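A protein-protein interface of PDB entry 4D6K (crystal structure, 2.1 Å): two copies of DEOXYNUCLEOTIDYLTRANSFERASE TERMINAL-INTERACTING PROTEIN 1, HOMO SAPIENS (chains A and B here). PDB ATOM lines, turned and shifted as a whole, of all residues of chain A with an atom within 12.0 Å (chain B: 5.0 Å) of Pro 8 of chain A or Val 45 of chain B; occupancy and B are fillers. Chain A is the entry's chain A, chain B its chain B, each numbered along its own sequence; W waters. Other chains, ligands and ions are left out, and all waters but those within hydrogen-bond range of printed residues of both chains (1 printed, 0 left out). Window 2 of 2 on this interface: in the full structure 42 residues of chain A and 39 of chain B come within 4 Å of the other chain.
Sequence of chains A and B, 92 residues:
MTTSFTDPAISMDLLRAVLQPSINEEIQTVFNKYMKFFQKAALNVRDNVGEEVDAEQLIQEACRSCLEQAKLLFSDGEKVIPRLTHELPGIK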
ATOM      1  N   ASP A   7      16.135  17.690   7.693  1.00  0.00           N
ATOM      2  CA  ASP A   7      15.358  17.514   6.441  1.00  0.00           C
ATOM      3  C   ASP A   7      16.151  18.221   5.312  1.00  0.00           C
ATOM      4  O   ASP A   7      16.422  19.421   5.411  1.00  0.00           O
ATOM      5  CB  ASP A   7      13.945  18.083   6.614  1.00  0.00           C
ATOM      6  CG  ASP A   7      13.153  18.150   5.301  1.00  0.00           C
ATOM      7  OD1 ASP A   7      13.476  17.466   4.308  1.00  0.00           O
ATOM      8  OD2 ASP A   7      12.185  18.913   5.274  1.00  0.00           O
ATOM      9  N   PRO A   8      16.576  17.476   4.264  1.00  0.00           N
ATOM     10  CA  PRO A   8      17.323  18.060   3.121  1.00  0.00           C
ATOM     11  C   PRO A   8      16.631  19.243   2.416  1.00  0.00           C
ATOM     12  O   PRO A   8      17.304  20.125   1.888  1.00  0.00           O
ATOM     13  CB  PRO A   8      17.406  16.906   2.131  1.00  0.00           C
ATOM     14  CG  PRO A   8      17.258  15.678   2.964  1.00  0.00           C
ATOM     15  CD  PRO A   8      16.307  16.045   4.050  1.00  0.00           C
ATOM     16  N   ALA A   9      15.296  19.273   2.413  1.00  0.00           N
ATOM     17  CA  ALA A   9      14.569  20.390   1.784  1.00  0.00           C
ATOM     18  C   ALA A   9      14.790  21.781   2.468  1.00  0.00           C
ATOM     19  O   ALA A   9      14.485  22.822   1.892  1.00  0.00           O
ATOM     20  CB  ALA A   9      13.100  20.058   1.653  1.00  0.00           C
ATOM     21  N   ILE A  10      15.389  21.797   3.651  1.00  0.00           N
ATOM     22  CA  ILE A  10      15.903  23.043   4.228  1.00  0.00           C
ATOM     23  C   ILE A  10      16.942  23.712   3.320  1.00  0.00           C
ATOM     24  O   ILE A  10      17.235  24.910   3.468  1.00  0.00           O
ATOM     25  CB  ILE A  10      16.436  22.804   5.654  1.00  0.00           C
ATOM     26  CG1 ILE A  10      16.506  24.102   6.531  1.00  0.00           C
ATOM     27  CG2 ILE A  10      17.721  22.026   5.551  1.00  0.00           C
ATOM     28  CD1 ILE A  10      17.749  24.952   6.378  1.00  0.00           C
ATOM     29  N   SER A  11      17.535  22.965   2.387  1.00  0.00           N
ATOM     30  CA  SER A  11      18.385  23.606   1.363  1.00  0.00           C
ATOM     31  C   SER A  11      17.604  24.671   0.582  1.00  0.00           C
ATOM     32  O   SER A  11      18.204  25.627   0.184  1.00  0.00           O
ATOM     33  CB  SER A  11      19.036  22.591   0.419  1.00  0.00           C
ATOM     34  OG  SER A  11      18.060  21.858  -0.304  1.00  0.00           O
ATOM     35  N   MET A  12      16.278  24.522   0.427  1.00  0.00           N
ATOM     36  CA  MET A  12      15.470  25.554  -0.213  1.00  0.00           C
ATOM     37  C   MET A  12      15.452  26.879   0.597  1.00  0.00           C
ATOM     38  O   MET A  12      15.633  27.938   0.015  1.00  0.00           O
ATOM     39  CB  MET A  12      14.045  25.112  -0.500  1.00  0.00           C
ATOM     40  CG  MET A  12      13.939  23.902  -1.447  1.00  0.00           C
ATOM     41  SD  MET A  12      14.679  24.077  -3.087  1.00  0.00           S
ATOM     42  CE  MET A  12      13.724  25.403  -3.778  1.00  0.00           C
ATOM     43  N   ASP A  13      15.294  26.777   1.896  1.00  0.00           N
ATOM     44  CA  ASP A  13      15.299  27.897   2.786  1.00  0.00           C
ATOM     45  C   ASP A  13      16.627  28.636   2.787  1.00  0.00           C
ATOM     46  O   ASP A  13      16.652  29.847   2.829  1.00  0.00           O
ATOM     47  CB  ASP A  13      15.063  27.448   4.235  1.00  0.00           C
ATOM     48  CG  ASP A  13      13.690  26.964   4.474  1.00  0.00           C
ATOM     49  OD1 ASP A  13      12.819  27.330   3.751  1.00  0.00           O
ATOM     50  OD2 ASP A  13      13.476  26.215   5.416  1.00  0.00           O
ATOM     51  N   LEU A  14      17.706  27.890   2.762  1.00  0.00           N
ATOM     52  CA  LEU A  14      18.964  28.516   2.784  1.00  0.00           C
ATOM     53  C   LEU A  14      19.252  29.264   1.515  1.00  0.00           C
ATOM     54  O   LEU A  14      19.792  30.339   1.567  1.00  0.00           O
ATOM     55  CB  LEU A  14      20.010  27.474   2.998  1.00  0.00           C
ATOM     56  CG  LEU A  14      21.432  27.909   3.257  1.00  0.00           C
ATOM     57  CD1 LEU A  14      21.533  28.973   4.344  1.00  0.00           C
ATOM     58  CD2 LEU A  14      22.249  26.661   3.611  1.00  0.00           C
ATOM     59  N   LEU A  15      18.899  28.666   0.374  1.00  0.00           N
ATOM     60  CA  LEU A  15      19.013  29.359  -0.877  1.00  0.00           C
ATOM     61  C   LEU A  15      18.167  30.620  -0.877  1.00  0.00           C
ATOM     62  O   LEU A  15      18.591  31.717  -1.322  1.00  0.00           O
ATOM     63  CB  LEU A  15      18.560  28.448  -2.035  1.00  0.00           C
ATOM     64  CG  LEU A  15      18.531  29.111  -3.395  1.00  0.00           C
ATOM     65  CD1 LEU A  15      19.935  29.606  -3.757  1.00  0.00           C
ATOM     66  CD2 LEU A  15      18.034  28.183  -4.490  1.00  0.00           C
ATOM     67  N   ARG A  16      16.949  30.478  -0.401  1.00  0.00           N
ATOM     68  CA  ARG A  16      16.037  31.596  -0.311  1.00  0.00           C
ATOM     69  C   ARG A  16      16.692  32.776   0.464  1.00  0.00           C
ATOM     70  O   ARG A  16      16.674  33.934   0.004  1.00  0.00           O
ATOM     71  CB  ARG A  16      14.751  31.153   0.384  1.00  0.00           C
ATOM     72  CG  ARG A  16      13.519  31.924  -0.004  1.00  0.00           C
ATOM     73  CD  ARG A  16      12.844  32.334   1.264  1.00  0.00           C
ATOM     74  NE  ARG A  16      12.589  31.124   2.046  1.00  0.00           N
ATOM     75  CZ  ARG A  16      12.642  31.133   3.371  1.00  0.00           C
ATOM     76  NH1 ARG A  16      12.879  32.299   3.975  1.00  0.00           N
ATOM     77  NH2 ARG A  16      12.475  30.019   4.066  1.00  0.00           N
ATOM     78  N   ALA B  41      18.025  23.832  -7.262  1.00  0.00           N
ATOM     79  CA  ALA B  41      18.049  23.383  -5.858  1.00  0.00           C
ATOM     80  C   ALA B  41      16.928  22.377  -5.593  1.00  0.00           C
ATOM     81  O   ALA B  41      17.109  21.401  -4.854  1.00  0.00           O
ATOM     82  CB  ALA B  41      17.943  24.557  -4.933  1.00  0.00           C
ATOM     83  N   ALA B  42      15.736  22.621  -6.127  1.00  0.00           N
ATOM     84  CA  ALA B  42      14.613  21.688  -5.892  1.00  0.00           C
ATOM     85  C   ALA B  42      14.829  20.307  -6.587  1.00  0.00           C
ATOM     86  O   ALA B  42      14.560  19.250  -6.005  1.00  0.00           O
ATOM     87  CB  ALA B  42      13.311  22.273  -6.409  1.00  0.00           C
ATOM     88  N   LEU B  43      15.365  20.330  -7.791  1.00  0.00           N
ATOM     89  CA  LEU B  43      15.792  19.089  -8.479  1.00  0.00           C
ATOM     90  C   LEU B  43      16.886  18.359  -7.689  1.00  0.00           C
ATOM     91  O   LEU B  43      16.827  17.160  -7.538  1.00  0.00           O
ATOM     92  CB  LEU B  43      16.289  19.361  -9.901  1.00  0.00           C
ATOM     93  CG  LEU B  43      15.128  19.800 -10.809  1.00  0.00           C
ATOM     94  CD1 LEU B  43      15.651  20.286 -12.162  1.00  0.00           C
ATOM     95  CD2 LEU B  43      14.062  18.729 -11.002  1.00  0.00           C
ATOM     96  N   ASN B  44      17.863  19.092  -7.172  1.00  0.00           N
ATOM     97  CA  ASN B  44      18.839  18.498  -6.285  1.00  0.00           C
ATOM     98  C   ASN B  44      18.228  17.762  -5.109  1.00  0.00           C
ATOM     99  O   ASN B  44      18.691  16.690  -4.744  1.00  0.00           O
ATOM    100  CB  ASN B  44      19.810  19.538  -5.831  1.00  0.00           C
ATOM    101  CG  ASN B  44      20.995  18.936  -5.071  1.00  0.00           C
ATOM    102  OD1 ASN B  44      21.753  18.194  -5.656  1.00  0.00           O
ATOM    103  ND2 ASN B  44      21.144  19.239  -3.790  1.00  0.00           N
ATOM    104  N   VAL B  45      17.240  18.375  -4.463  1.00  0.00           N
ATOM    105  CA  VAL B  45      16.620  17.723  -3.371  1.00  0.00           C
ATOM    106  C   VAL B  45      15.938  16.426  -3.878  1.00  0.00           C
ATOM    107  O   VAL B  45      16.072  15.378  -3.254  1.00  0.00           O
ATOM    108  CB  VAL B  45      15.622  18.655  -2.626  1.00  0.00           C
ATOM    109  CG1 VAL B  45      14.864  17.873  -1.600  1.00  0.00           C
ATOM    110  CG2 VAL B  45      16.357  19.793  -1.930  1.00  0.00           C
ATOM    111  N   ARG B  46      15.203  16.507  -4.980  1.00  0.00           N
ATOM    112  CA  ARG B  46      14.496  15.344  -5.466  1.00  0.00           C
ATOM    113  C   ARG B  46      15.449  14.203  -5.890  1.00  0.00           C
ATOM    114  O   ARG B  46      15.174  13.043  -5.660  1.00  0.00           O
ATOM    115  CB  ARG B  46      13.614  15.710  -6.632  1.00  0.00           C
ATOM    116  CG  ARG B  46      12.807  14.543  -7.139  1.00  0.00           C
ATOM    117  CD  ARG B  46      11.937  14.987  -8.285  1.00  0.00           C
ATOM    118  NE  ARG B  46      12.733  15.047  -9.490  1.00  0.00           N
ATOM    119  CZ  ARG B  46      12.333  15.592 -10.640  1.00  0.00           C
ATOM    120  NH1 ARG B  46      11.123  16.127 -10.745  1.00  0.00           N
ATOM    121  NH2 ARG B  46      13.159  15.584 -11.687  1.00  0.00           N
ATOM    122  N   ASP B  47      16.531  14.578  -6.532  1.00  0.00           N
ATOM    123  CA  ASP B  47      17.565  13.666  -6.965  1.00  0.00           C
ATOM    124  C   ASP B  47      18.205  12.931  -5.801  1.00  0.00           C
ATOM    125  O   ASP B  47      18.581  11.779  -5.949  1.00  0.00           O
ATOM    126  CB  ASP B  47      18.700  14.397  -7.708  1.00  0.00           C
ATOM    127  CG  ASP B  47      18.266  15.016  -9.011  1.00  0.00           C
ATOM    128  OD1 ASP B  47      17.252  14.557  -9.555  1.00  0.00           O
ATOM    129  OD2 ASP B  47      18.991  15.928  -9.475  1.00  0.00           O
ATOM    130  N   ASN B  48      18.285  13.556  -4.639  1.00  0.00           N
ATOM    131  CA  ASN B  48      18.911  12.938  -3.481  1.00  0.00           C
ATOM    132  C   ASN B  48      17.895  12.155  -2.667  1.00  0.00           C
ATOM    133  O   ASN B  48      18.134  11.028  -2.256  1.00  0.00           O
ATOM    134  CB  ASN B  48      19.734  13.999  -2.695  1.00  0.00           C
ATOM    135  CG  ASN B  48      21.047  14.302  -3.356  1.00  0.00           C
ATOM    136  OD1 ASN B  48      21.985  13.520  -3.275  1.00  0.00           O
ATOM    137  ND2 ASN B  48      21.112  15.407  -4.100  1.00  0.00           N
ATOM    138  N   VAL B  49      16.709  12.710  -2.487  1.00  0.00           N
ATOM    139  CA  VAL B  49      15.726  12.118  -1.579  1.00  0.00           C
ATOM    140  C   VAL B  49      14.839  11.129  -2.247  1.00  0.00           C
ATOM    141  O   VAL B  49      14.530  10.140  -1.624  1.00  0.00           O
ATOM    142  CB  VAL B  49      14.885  13.198  -0.855  1.00  0.00           C
ATOM    143  CG1 VAL B  49      13.934  12.579   0.149  1.00  0.00           C
ATOM    144  CG2 VAL B  49      15.794  14.179  -0.134  1.00  0.00           C
ATOM    145  N   GLY B  50      14.404  11.391  -3.470  1.00  0.00           N
ATOM    146  CA  GLY B  50      13.479  10.454  -4.145  1.00  0.00           C
ATOM    147  C   GLY B  50      12.223  11.020  -4.754  1.00  0.00           C
ATOM    148  O   GLY B  50      11.909  12.193  -4.622  1.00  0.00           O
ATOM    149  N   VAL B  53       9.357  13.558  -3.432  1.00  0.00           N
ATOM    150  CA  VAL B  53       9.580  14.990  -3.341  1.00  0.00           C
ATOM    151  C   VAL B  53       8.957  15.617  -4.595  1.00  0.00           C
ATOM    152  O   VAL B  53       9.271  15.241  -5.708  1.00  0.00           O
ATOM    153  CB  VAL B  53      11.077  15.320  -3.346  1.00  0.00           C
ATOM    154  CG1 VAL B  53      11.332  16.777  -3.723  1.00  0.00           C
ATOM    155  CG2 VAL B  53      11.692  15.011  -2.011  1.00  0.00           C
ATOM    156  N   LEU B  58       8.199  22.581  -4.144  1.00  0.00           N
ATOM    157  CA  LEU B  58       9.276  23.205  -3.379  1.00  0.00           C
ATOM    158  C   LEU B  58       9.584  24.564  -3.965  1.00  0.00           C
ATOM    159  O   LEU B  58       9.861  25.481  -3.255  1.00  0.00           O
ATOM    160  CB  LEU B  58      10.546  22.347  -3.427  1.00  0.00           C
ATOM    161  CG  LEU B  58      10.538  21.020  -2.677  1.00  0.00           C
ATOM    162  CD1 LEU B  58      11.902  20.343  -2.885  1.00  0.00           C
ATOM    163  CD2 LEU B  58      10.254  21.191  -1.196  1.00  0.00           C
HETATM  164  O   HOH W   1      19.131  21.509  -2.770  1.00  0.00           O
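The backbone carbonyl oxygen (O) of Pro 8 of chain A is in hydrogen-bond range of the side-chain hydroxyl (OG) of Ser 11 of chain A, at 2.9 Å.
Pro 8 of chain A touches Val 45 of chain B (O to CG2, 3.9 Å). CG2 of Val 49 of chain B touches CG of Pro 8 of chain A, at 3.7 Å. OG of Ser 11 of chain A touches CG2 of Val 45 of chain B, 3.1 Å away. SD of Met 12 of chain A touches C of Ala 41 of chain B (3.8 Å). Leu 58 of chain B touches Met 12 of chain A. Leu 15 of chain A touches Ala 41 of chain B.
No position is printed for both chains.
Pro 8 of chain A touches just these residues of chain B: Val 45 (3.9 Å) and Val 49 (3.7 Å). Ile 10 of chain A touches none of the printed residues of chain B. Of the printed residues of chain B, Ser 11 of chain A touches Val 45. Of the printed residues of chain B, Met 12 of chain A touches Ala 41, Ala 42 and Leu 58. Of the printed residues of chain B, Leu 15 of chain A touches Ala 41. Ala 41 of chain B touches two residues of chain A. Ala 42 of chain B touches just one residue of chain A: Met 12 (3.5 Å). Leu 43 of chain B touches none of the printed residues of chain A. Asn 44 of chain B touches none of the printed residues of chain A. Of chain A, only Pro 8 and Ser 11 come within 4 Å of Val 45 of chain B. No residue of chain A comes within 4 Å of Asp 47 of chain B. No residue of chain A comes within 4 Å of Asn 48 of chain B. Gly 50 of chain B touches none of the printed residues of chain A. Val 53 of chain B touches none of the printed residues of chain A. Printed residues of chain A within 4 Å of Leu 58 of chain B: Met 12. The nearest printed residue of chain B that does not touch Ser 11 of chain A is Ala 41 of chain B (4.7 Å).
Water W1 lies within hydrogen-bond range of OG of Ser 11 of chain A (2.7 Å), O of Ala 41 of chain B (2.9 Å) and ND2 of Asn 44 of chain B (3.2 Å).
Printed residues of chain B that touch a printed residue of chain A: Ala 41, Ala 42, Val 45, Val 49 and Leu 58. Hydrophobic or aromatic side chains of chain A within 4 Å of the printed part of chain B: Pro 8, Met 12 and Leu 15. Along chain A the printed residues that touch a printed residue of chain B span positions 8 to 15. Among the printed residues, 7 pairs touch across the chains.
The side-chain sulfur of Met 12 of chain A lies within hydrogen-bond range of the backbone NH of Ala 42 of chain B (3.5 Å).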
